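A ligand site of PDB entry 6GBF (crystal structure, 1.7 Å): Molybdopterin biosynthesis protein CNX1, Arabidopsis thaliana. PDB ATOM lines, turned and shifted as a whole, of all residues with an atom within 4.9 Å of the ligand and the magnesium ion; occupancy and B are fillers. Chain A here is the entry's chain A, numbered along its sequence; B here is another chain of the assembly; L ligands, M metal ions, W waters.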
ATOM      1  N   SER A 197      14.835   8.678  -1.586  1.00  0.00           N
ATOM      2  CA  SER A 197      13.759   9.031  -0.658  1.00  0.00           C
ATOM      3  C   SER A 197      13.468  10.489  -0.842  1.00  0.00           C
ATOM      4  O   SER A 197      14.349  11.243  -1.265  1.00  0.00           O
ATOM      5  CB  SER A 197      14.179   8.786   0.789  1.00  0.00           C
ATOM      6  OG  SER A 197      14.104   7.394   1.015  1.00  0.00           O
ATOM      7  N   THR A 198      12.250  10.911  -0.496  1.00  0.00           N
ATOM      8  CA  THR A 198      11.903  12.332  -0.564  1.00  0.00           C
ATOM      9  C   THR A 198      11.330  12.813   0.761  1.00  0.00           C
ATOM     10  O   THR A 198      10.626  12.077   1.451  1.00  0.00           O
ATOM     11  CB  THR A 198      10.917  12.612  -1.706  1.00  0.00           C
ATOM     12  OG1 THR A 198       9.624  12.093  -1.381  1.00  0.00           O
ATOM     13  CG2 THR A 198      11.413  12.069  -3.082  1.00  0.00           C
ATOM     14  N   GLY A 199      11.623  14.060   1.099  1.00  0.00           N
ATOM     15  CA  GLY A 199      11.023  14.692   2.262  1.00  0.00           C
ATOM     16  C   GLY A 199      11.899  15.629   3.048  1.00  0.00           C
ATOM     17  O   GLY A 199      12.993  15.265   3.454  1.00  0.00           O
ATOM     18  N   GLU A 201      11.229  16.351   6.070  1.00  0.00           N
ATOM     19  CA  GLU A 201      11.204  15.806   7.430  1.00  0.00           C
ATOM     20  C   GLU A 201      12.234  14.682   7.629  1.00  0.00           C
ATOM     21  O   GLU A 201      12.453  14.285   8.760  1.00  0.00           O
ATOM     22  CB  GLU A 201       9.786  15.301   7.823  1.00  0.00           C
ATOM     23  CG  GLU A 201       9.347  13.921   7.311  1.00  0.00           C
ATOM     24  CD  GLU A 201       8.963  13.836   5.854  1.00  0.00           C
ATOM     25  OE1 GLU A 201       9.279  14.769   5.090  1.00  0.00           O
ATOM     26  OE2 GLU A 201       8.328  12.835   5.465  1.00  0.00           O
ATOM     27  N   LEU A 202      12.853  14.165   6.575  1.00  0.00           N
ATOM     28  CA  LEU A 202      13.774  13.038   6.720  1.00  0.00           C
ATOM     29  C   LEU A 202      15.169  13.440   7.160  1.00  0.00           C
ATOM     30  O   LEU A 202      15.677  14.485   6.734  1.00  0.00           O
ATOM     31  CB  LEU A 202      13.912  12.264   5.406  1.00  0.00           C
ATOM     32  CG  LEU A 202      12.608  11.770   4.751  1.00  0.00           C
ATOM     33  CD1 LEU A 202      12.916  11.087   3.445  1.00  0.00           C
ATOM     34  CD2 LEU A 202      11.836  10.827   5.693  1.00  0.00           C
ATOM     35  N   ILE A 215      12.184  12.577  11.226  1.00  0.00           N
ATOM     36  CA  ILE A 215      12.165  11.119  11.346  1.00  0.00           C
ATOM     37  C   ILE A 215      13.354  10.581  10.562  1.00  0.00           C
ATOM     38  O   ILE A 215      13.743  11.182   9.555  1.00  0.00           O
ATOM     39  CB  ILE A 215      10.857  10.465  10.838  1.00  0.00           C
ATOM     40  CG1 ILE A 215      10.564  10.821   9.342  1.00  0.00           C
ATOM     41  CG2 ILE A 215       9.677  10.870  11.728  1.00  0.00           C
ATOM     42  CD1 ILE A 215       9.538   9.912   8.670  1.00  0.00           C
ATOM     43  N   ARG A 216      13.840   9.398  10.929  1.00  0.00           N
ATOM     44  CA  ARG A 216      14.911   8.761  10.151  1.00  0.00           C
ATOM     45  C   ARG A 216      14.338   8.205   8.843  1.00  0.00           C
ATOM     46  O   ARG A 216      13.219   7.679   8.811  1.00  0.00           O
ATOM     47  CB  ARG A 216      15.562   7.613  10.939  1.00  0.00           C
ATOM     48  CG  ARG A 216      16.325   8.138  12.154  1.00  0.00           C
ATOM     49  CD  ARG A 216      17.130   7.109  12.952  1.00  0.00           C
ATOM     50  NE  ARG A 216      17.533   7.716  14.234  1.00  0.00           N
ATOM     51  CZ  ARG A 216      16.787   7.771  15.332  1.00  0.00           C
ATOM     52  NH1 ARG A 216      15.616   7.132  15.379  1.00  0.00           N
ATOM     53  NH2 ARG A 216      17.220   8.436  16.402  1.00  0.00           N
ATOM     54  N   ASP A 217      15.104   8.363   7.754  1.00  0.00           N
ATOM     55  CA  ASP A 217      14.746   7.797   6.460  1.00  0.00           C
ATOM     56  C   ASP A 217      14.838   6.255   6.615  1.00  0.00           C
ATOM     57  O   ASP A 217      15.938   5.722   6.799  1.00  0.00           O
ATOM     58  CB  ASP A 217      15.760   8.282   5.399  1.00  0.00           C
ATOM     59  CG  ASP A 217      15.610   7.711   4.003  1.00  0.00           C
ATOM     60  OD1 ASP A 217      14.617   7.012   3.753  1.00  0.00           O
ATOM     61  OD2 ASP A 217      16.481   7.987   3.151  1.00  0.00           O
ATOM     62  N   SER A 218      13.701   5.558   6.589  1.00  0.00           N
ATOM     63  CA  SER A 218      13.684   4.096   6.696  1.00  0.00           C
ATOM     64  C   SER A 218      13.388   3.449   5.355  1.00  0.00           C
ATOM     65  O   SER A 218      13.837   2.326   5.115  1.00  0.00           O
ATOM     66  CB  SER A 218      12.668   3.634   7.754  1.00  0.00           C
ATOM     67  OG  SER A 218      11.326   3.951   7.445  1.00  0.00           O
ATOM     68  N   ASN A 219      12.610   4.103   4.479  1.00  0.00           N
ATOM     69  CA  ASN A 219      12.241   3.500   3.199  1.00  0.00           C
ATOM     70  C   ASN A 219      13.425   3.169   2.309  1.00  0.00           C
ATOM     71  O   ASN A 219      13.395   2.146   1.607  1.00  0.00           O
ATOM     72  CB  ASN A 219      11.261   4.389   2.411  1.00  0.00           C
ATOM     73  CG  ASN A 219       9.873   4.452   2.992  1.00  0.00           C
ATOM     74  OD1 ASN A 219       9.523   3.671   3.883  1.00  0.00           O
ATOM     75  ND2 ASN A 219       9.059   5.369   2.512  1.00  0.00           N
ATOM     76  N   ARG A 220      14.425   4.073   2.272  1.00  0.00           N
ATOM     77  CA  ARG A 220      15.560   3.868   1.374  1.00  0.00           C
ATOM     78  C   ARG A 220      16.341   2.605   1.707  1.00  0.00           C
ATOM     79  O   ARG A 220      16.492   1.753   0.837  1.00  0.00           O
ATOM     80  CB  ARG A 220      16.494   5.107   1.381  1.00  0.00           C
ATOM     81  CG  ARG A 220      17.626   5.053   0.324  1.00  0.00           C
ATOM     82  CD  ARG A 220      18.057   6.487  -0.004  1.00  0.00           C
ATOM     83  NE  ARG A 220      18.271   7.252   1.237  1.00  0.00           N
ATOM     84  CZ  ARG A 220      19.391   7.366   1.936  1.00  0.00           C
ATOM     85  NH1 ARG A 220      20.544   6.900   1.442  1.00  0.00           N
ATOM     86  NH2 ARG A 220      19.396   8.027   3.078  1.00  0.00           N
ATOM     87  N   ASP A 242      11.865  18.428  -0.678  1.00  0.00           N
ATOM     88  CA  ASP A 242      10.596  18.729  -1.357  1.00  0.00           C
ATOM     89  C   ASP A 242      10.742  20.045  -2.128  1.00  0.00           C
ATOM     90  O   ASP A 242      10.166  21.069  -1.790  1.00  0.00           O
ATOM     91  CB  ASP A 242       9.436  18.740  -0.339  1.00  0.00           C
ATOM     92  CG  ASP A 242       9.271  17.407   0.399  1.00  0.00           C
ATOM     93  OD1 ASP A 242       9.381  16.333  -0.256  1.00  0.00           O
ATOM     94  OD2 ASP A 242       9.044  17.436   1.628  1.00  0.00           O
ATOM     95  N   SER A 265      10.168   7.112  -3.178  1.00  0.00           N
ATOM     96  CA  SER A 265       9.095   6.918  -2.201  1.00  0.00           C
ATOM     97  C   SER A 265       8.713   8.300  -1.676  1.00  0.00           C
ATOM     98  O   SER A 265       9.552   9.191  -1.676  1.00  0.00           O
ATOM     99  CB  SER A 265       9.473   5.946  -1.079  1.00  0.00           C
ATOM    100  OG  SER A 265      10.294   6.504  -0.071  1.00  0.00           O
ATOM    101  N   GLY A 266       7.461   8.496  -1.326  1.00  0.00           N
ATOM    102  CA  GLY A 266       6.958   9.762  -0.812  1.00  0.00           C
ATOM    103  C   GLY A 266       6.757  10.769  -1.924  1.00  0.00           C
ATOM    104  O   GLY A 266       7.052  10.473  -3.087  1.00  0.00           O
ATOM    105  N   GLY A 267       6.245  11.969  -1.582  1.00  0.00           N
ATOM    106  CA  GLY A 267       6.050  13.016  -2.573  1.00  0.00           C
ATOM    107  C   GLY A 267       5.012  12.708  -3.638  1.00  0.00           C
ATOM    108  O   GLY A 267       5.068  13.285  -4.733  1.00  0.00           O
ATOM    109  N   VAL A 268       4.092  11.766  -3.342  1.00  0.00           N
ATOM    110  CA  VAL A 268       3.052  11.309  -4.280  1.00  0.00           C
ATOM    111  C   VAL A 268       1.671  11.409  -3.667  1.00  0.00           C
ATOM    112  O   VAL A 268       0.750  10.834  -4.219  1.00  0.00           O
ATOM    113  CB  VAL A 268       3.291   9.850  -4.817  1.00  0.00           C
ATOM    114  CG1 VAL A 268       4.363   9.837  -5.895  1.00  0.00           C
ATOM    115  CG2 VAL A 268       3.624   8.878  -3.692  1.00  0.00           C
ATOM    116  N   SER A 269       1.477  12.131  -2.550  1.00  0.00           N
ATOM    117  CA  SER A 269       0.151  12.252  -1.949  1.00  0.00           C
ATOM    118  C   SER A 269      -0.517  13.547  -2.506  1.00  0.00           C
ATOM    119  O   SER A 269      -0.291  13.888  -3.667  1.00  0.00           O
ATOM    120  CB  SER A 269       0.216  12.226  -0.414  1.00  0.00           C
ATOM    121  OG  SER A 269       0.898  11.102   0.107  1.00  0.00           O
ATOM    122  N   ASP A 274       4.479  17.910  -3.203  1.00  0.00           N
ATOM    123  CA  ASP A 274       4.589  16.525  -3.696  1.00  0.00           C
ATOM    124  C   ASP A 274       4.802  16.638  -5.204  1.00  0.00           C
ATOM    125  O   ASP A 274       3.844  16.888  -5.935  1.00  0.00           O
ATOM    126  CB  ASP A 274       3.279  15.769  -3.378  1.00  0.00           C
ATOM    127  CG  ASP A 274       3.189  15.341  -1.925  1.00  0.00           C
ATOM    128  OD1 ASP A 274       4.184  15.499  -1.193  1.00  0.00           O
ATOM    129  OD2 ASP A 274       2.143  14.812  -1.529  1.00  0.00           O
ATOM    130  N   GLY A 324       4.881   7.014   0.310  1.00  0.00           N
ATOM    131  CA  GLY A 324       5.810   7.298   1.414  1.00  0.00           C
ATOM    132  C   GLY A 324       5.586   6.437   2.645  1.00  0.00           C
ATOM    133  O   GLY A 324       6.539   6.110   3.353  1.00  0.00           O
ATOM    134  N   ASN A 325       4.322   6.114   2.971  1.00  0.00           N
ATOM    135  CA  ASN A 325       4.049   5.289   4.154  1.00  0.00           C
ATOM    136  C   ASN A 325       4.843   3.967   4.099  1.00  0.00           C
ATOM    137  O   ASN A 325       4.759   3.273   3.093  1.00  0.00           O
ATOM    138  CB  ASN A 325       2.567   5.025   4.315  1.00  0.00           C
ATOM    139  CG  ASN A 325       1.822   6.161   4.976  1.00  0.00           C
ATOM    140  OD1 ASN A 325       2.215   6.653   6.057  1.00  0.00           O
ATOM    141  ND2 ASN A 325       0.721   6.593   4.373  1.00  0.00           N
ATOM    142  N   PRO A 326       5.691   3.674   5.104  1.00  0.00           N
ATOM    143  CA  PRO A 326       6.556   2.468   5.032  1.00  0.00           C
ATOM    144  C   PRO A 326       5.895   1.163   4.639  1.00  0.00           C
ATOM    145  O   PRO A 326       6.440   0.432   3.847  1.00  0.00           O
ATOM    146  CB  PRO A 326       7.116   2.378   6.452  1.00  0.00           C
ATOM    147  CG  PRO A 326       7.270   3.800   6.838  1.00  0.00           C
ATOM    148  CD  PRO A 326       6.013   4.468   6.320  1.00  0.00           C
ATOM    149  N   SER B  64       0.426  14.469  11.056  1.00  0.00           N
ATOM    150  CA  SER B  64      -0.777  14.368  10.223  1.00  0.00           C
ATOM    151  C   SER B  64      -0.749  13.121   9.362  1.00  0.00           C
ATOM    152  O   SER B  64       0.291  12.778   8.801  1.00  0.00           O
ATOM    153  CB  SER B  64      -0.906  15.586   9.322  1.00  0.00           C
ATOM    154  OG  SER B  64      -2.130  15.495   8.620  1.00  0.00           O
ATOM    155  N   ASP B  67      -3.009  15.301   3.905  1.00  0.00           N
ATOM    156  CA  ASP B  67      -2.748  16.617   3.373  1.00  0.00           C
ATOM    157  C   ASP B  67      -4.071  17.338   3.599  1.00  0.00           C
ATOM    158  O   ASP B  67      -5.105  16.848   3.156  1.00  0.00           O
ATOM    159  CB  ASP B  67      -2.409  16.551   1.886  1.00  0.00           C
ATOM    160  CG  ASP B  67      -1.216  15.647   1.653  1.00  0.00           C
ATOM    161  OD1 ASP B  67      -0.108  16.023   2.079  1.00  0.00           O
ATOM    162  OD2 ASP B  67      -1.393  14.553   1.096  1.00  0.00           O
ATOM    163  N   THR B 107       0.855  15.350   4.795  1.00  0.00           N
ATOM    164  CA  THR B 107       0.997  14.049   5.455  1.00  0.00           C
ATOM    165  C   THR B 107       2.408  13.968   6.050  1.00  0.00           C
ATOM    166  O   THR B 107       3.371  14.327   5.372  1.00  0.00           O
ATOM    167  CB  THR B 107       0.762  12.903   4.448  1.00  0.00           C
ATOM    168  OG1 THR B 107      -0.528  13.100   3.862  1.00  0.00           O
ATOM    169  CG2 THR B 107       0.831  11.524   5.094  1.00  0.00           C
ATOM    170  N   GLY B 108       2.505  13.618   7.336  1.00  0.00           N
ATOM    171  CA  GLY B 108       3.776  13.572   8.065  1.00  0.00           C
ATOM    172  C   GLY B 108       4.172  14.907   8.675  1.00  0.00           C
ATOM    173  O   GLY B 108       5.167  14.961   9.395  1.00  0.00           O
ATOM    174  N   ARG B 150      -1.572  10.927  13.951  1.00  0.00           N
ATOM    175  CA  ARG B 150      -0.802   9.852  14.558  1.00  0.00           C
ATOM    176  C   ARG B 150      -0.190  10.468  15.808  1.00  0.00           C
ATOM    177  O   ARG B 150       0.711  11.307  15.705  1.00  0.00           O
ATOM    178  CB  ARG B 150       0.332   9.378  13.638  1.00  0.00           C
ATOM    179  CG  ARG B 150      -0.155   8.552  12.443  1.00  0.00           C
ATOM    180  CD  ARG B 150       0.850   8.622  11.303  1.00  0.00           C
ATOM    181  NE  ARG B 150       2.118   8.011  11.715  1.00  0.00           N
ATOM    182  CZ  ARG B 150       3.341   8.409  11.395  1.00  0.00           C
ATOM    183  NH1 ARG B 150       3.524   9.471  10.606  1.00  0.00           N
ATOM    184  NH2 ARG B 150       4.408   7.758  11.859  1.00  0.00           N
HETATM  185  P1  LIG L   1       4.391  11.695   1.528  1.00  0.00           P
HETATM  186  O1  LIG L   1       3.460  12.729   2.183  1.00  0.00           O
HETATM  187  O2  LIG L   1       5.716  12.306   1.147  1.00  0.00           O
HETATM  188  O3  LIG L   1       3.739  10.871   0.487  1.00  0.00           O
HETATM  189  O4  LIG L   1       4.703  10.680   2.745  1.00  0.00           O
HETATM  190  C1  LIG L   1       3.674   9.903   3.340  1.00  0.00           C
HETATM  191  C2  LIG L   1       4.083   9.479   4.742  1.00  0.00           C
HETATM  192  O5  LIG L   1       5.231   8.608   4.645  1.00  0.00           O
HETATM  193  C3  LIG L   1       4.481  10.641   5.658  1.00  0.00           C
HETATM  194  O6  LIG L   1       4.005  10.331   6.977  1.00  0.00           O
HETATM  195  C4  LIG L   1       6.010  10.624   5.619  1.00  0.00           C
HETATM  196  O7  LIG L   1       6.647  11.193   6.768  1.00  0.00           O
HETATM  197  C5  LIG L   1       6.295   9.128   5.430  1.00  0.00           C
HETATM  198  N1  LIG L   1       7.572   8.942   4.712  1.00  0.00           N
HETATM  199  C6  LIG L   1       7.884   9.441   3.487  1.00  0.00           C
HETATM  200  N2  LIG L   1       9.131   9.045   3.117  1.00  0.00           N
HETATM  201  C7  LIG L   1       9.593   8.263   4.109  1.00  0.00           C
HETATM  202  C8  LIG L   1      10.844   7.522   4.373  1.00  0.00           C
HETATM  203  N3  LIG L   1      11.828   7.546   3.478  1.00  0.00           N
HETATM  204  N4  LIG L   1      10.953   6.804   5.500  1.00  0.00           N
HETATM  205  C9  LIG L   1       9.959   6.759   6.402  1.00  0.00           C
HETATM  206  N5  LIG L   1       8.791   7.419   6.239  1.00  0.00           N
HETATM  207  C10 LIG L   1       8.570   8.178   5.139  1.00  0.00           C
HETATM  208 MG    MG M   1       6.875  13.809   1.938  1.00  0.00          MG
HETATM  209  O   HOH W   1       5.970  11.053   9.575  1.00  0.00           O
HETATM  210  O   HOH W   2       8.163  12.429   2.795  1.00  0.00           O
HETATM  211  O   HOH W   3       2.724   8.630  -0.342  1.00  0.00           O
HETATM  212  O   HOH W   4       4.112   7.599   7.660  1.00  0.00           O
HETATM  213  O   HOH W   5       5.778  13.744   3.771  1.00  0.00           O
HETATM  214  O   HOH W   6      10.903   8.880   0.968  1.00  0.00           O
HETATM  215  O   HOH W   7       7.739   6.754   8.795  1.00  0.00           O
HETATM  216  O   HOH W   8       8.047  13.918   0.239  1.00  0.00           O
HETATM  217  O   HOH W   9       2.279  14.903   1.156  1.00  0.00           O
HETATM  218  O   HOH W  10       7.762  15.441   2.960  1.00  0.00           O
HETATM  219  O   HOH W  11       5.569  15.217   1.152  1.00  0.00           O
HETATM  220  O   HOH W  12       1.667  10.452   8.447  1.00  0.00           O
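The magnesium ion is bound by an oxygen (O2) of the ligand, water W8, water W2, water W11, water W10 and water W5.
N3 of the ligand sits at hydrogen-bond distance from OD1 of Asp 217 (2.9 Å).
The backbone NH of Asn 219 sits at hydrogen-bond distance from a nitrogen (N4) of the ligand, at 3.3 Å.
The side-chain carboxylate (OE2) of Glu 201 is in hydrogen-bond range of an oxygen (O7) of the ligand (2.7 Å).
The backbone NH (N) of Asn 325 lies within hydrogen-bond range of an oxygen (O5) of the ligand (3.1 Å).
OG of Ser 218 lies close to N4 of the ligand.
N of Gly 267 lies within hydrogen-bond range of O3 of the ligand.
The backbone NH (N) of Ser 218 sits at hydrogen-bond distance from a nitrogen (N4) of the ligand (3.2 Å).
A nitrogen (N3) of the ligand is in hydrogen-bond range of the side-chain hydroxyl of Ser 197, 3.4 Å away.
The side-chain hydroxyl (OG) of Ser 269 is in hydrogen-bond range of an oxygen (O3) of the ligand, 2.9 Å away.
O5 of the ligand sits close to O of Gly 324, at 3.1 Å.
Thr 198 touches the ligand (O to N2, 3.8 Å).
Leu 202 touches the ligand.
CD1 of Ile 215 touches N5 of the ligand (3.6 Å).
CA of Gly 266 touches O2 of the ligand (3.4 Å).
N of Val 268 touches O3 of the ligand, at 3.9 Å.
Pro 326 touches the ligand.
Thr 107 of chain B touches the ligand.
Gly 108 of chain B touches the ligand (CA to O6, 3.4 Å).
Arg 150 of chain B touches the ligand (NH1 to O6, 3.8 Å).
Hydrophobic or aromatic side chains that line the ligand: Leu 202, Ile 215 and Pro 326.
Within 4 Å of the ligand: Ser 197, Thr 198, Glu 201, Leu 202, Ile 215, Asp 217, Ser 218, Asn 219, Gly 266, Gly 267, Val 268, Ser 269, Gly 324, Asn 325, Pro 326, Thr 107 of chain B, Gly 108 of chain B and Arg 150 of chain B.
The backbone NH of Ser 269 lies within hydrogen-bond range of the side-chain carboxylate of Asp 274 (2.9 Å).
The backbone carbonyl oxygen of Ser 265 sits at hydrogen-bond distance from the side-chain hydroxyl of Thr 198 (2.9 Å).
The backbone carbonyl oxygen of Gly 324 sits at hydrogen-bond distance from the side-chain amide nitrogen of Asn 219 (2.8 Å).
The backbone NH of Gly 108 of chain B sits at hydrogen-bond distance from the backbone carbonyl oxygen of Ser 64 of chain B (2.8 Å).
N of Thr 107 of chain B sits at hydrogen-bond distance from OD1 of Asp 67 of chain B (3.0 Å).
The backbone carbonyl oxygen (O) of Glu 201 lies within hydrogen-bond range of the backbone NH (N) of Ile 215 (3.0 Å).
The side-chain carboxylate of Asp 217 is in hydrogen-bond range of the side-chain hydroxyl of Ser 197 (2.8 Å).
The side-chain amide nitrogen of Asn 219 is in hydrogen-bond range of the side-chain hydroxyl of Ser 265 (3.1 Å).
Water W10 lies within hydrogen-bond range of the side-chain carboxylate of Glu 201 (2.7 Å) and the side-chain carboxylate of Asp 242 (2.7 Å).
Water W8 lies within hydrogen-bond range of OD1 of Asp 242 (2.8 Å), OG1 of Thr 198 (2.9 Å) and N of Gly 267 (3.2 Å).
Water W11 bridges OD1 of Asp 274 (2.7 Å) and O1 of the ligand (3.4 Å).
Water W9 lies within hydrogen-bond range of an oxygen (O1) of the ligand, the side-chain carboxylate (OD2) of Asp 274 and the side-chain carboxylate (OD1) of Asp 67 of chain B.
Water W12 lies within hydrogen-bond range of O of Ser 64 of chain B (2.7 Å), O6 of the ligand (2.8 Å), NH1 of Arg 150 of chain B (3.0 Å) and N of Gly 108 of chain B (3.5 Å).
Water W6 lies within hydrogen-bond range of OG of Ser 265 (2.7 Å), N2 of the ligand (2.8 Å) and N of Thr 198 (2.8 Å).
OE2 of Glu 201 touches the magnesium ion, at 3.9 Å.
Of the 26 residues printed, 1 comes within 4 Å of the magnesium ion.
The nearest printed residue that does not touch the magnesium ion is Gly 267 (4.02 Å).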
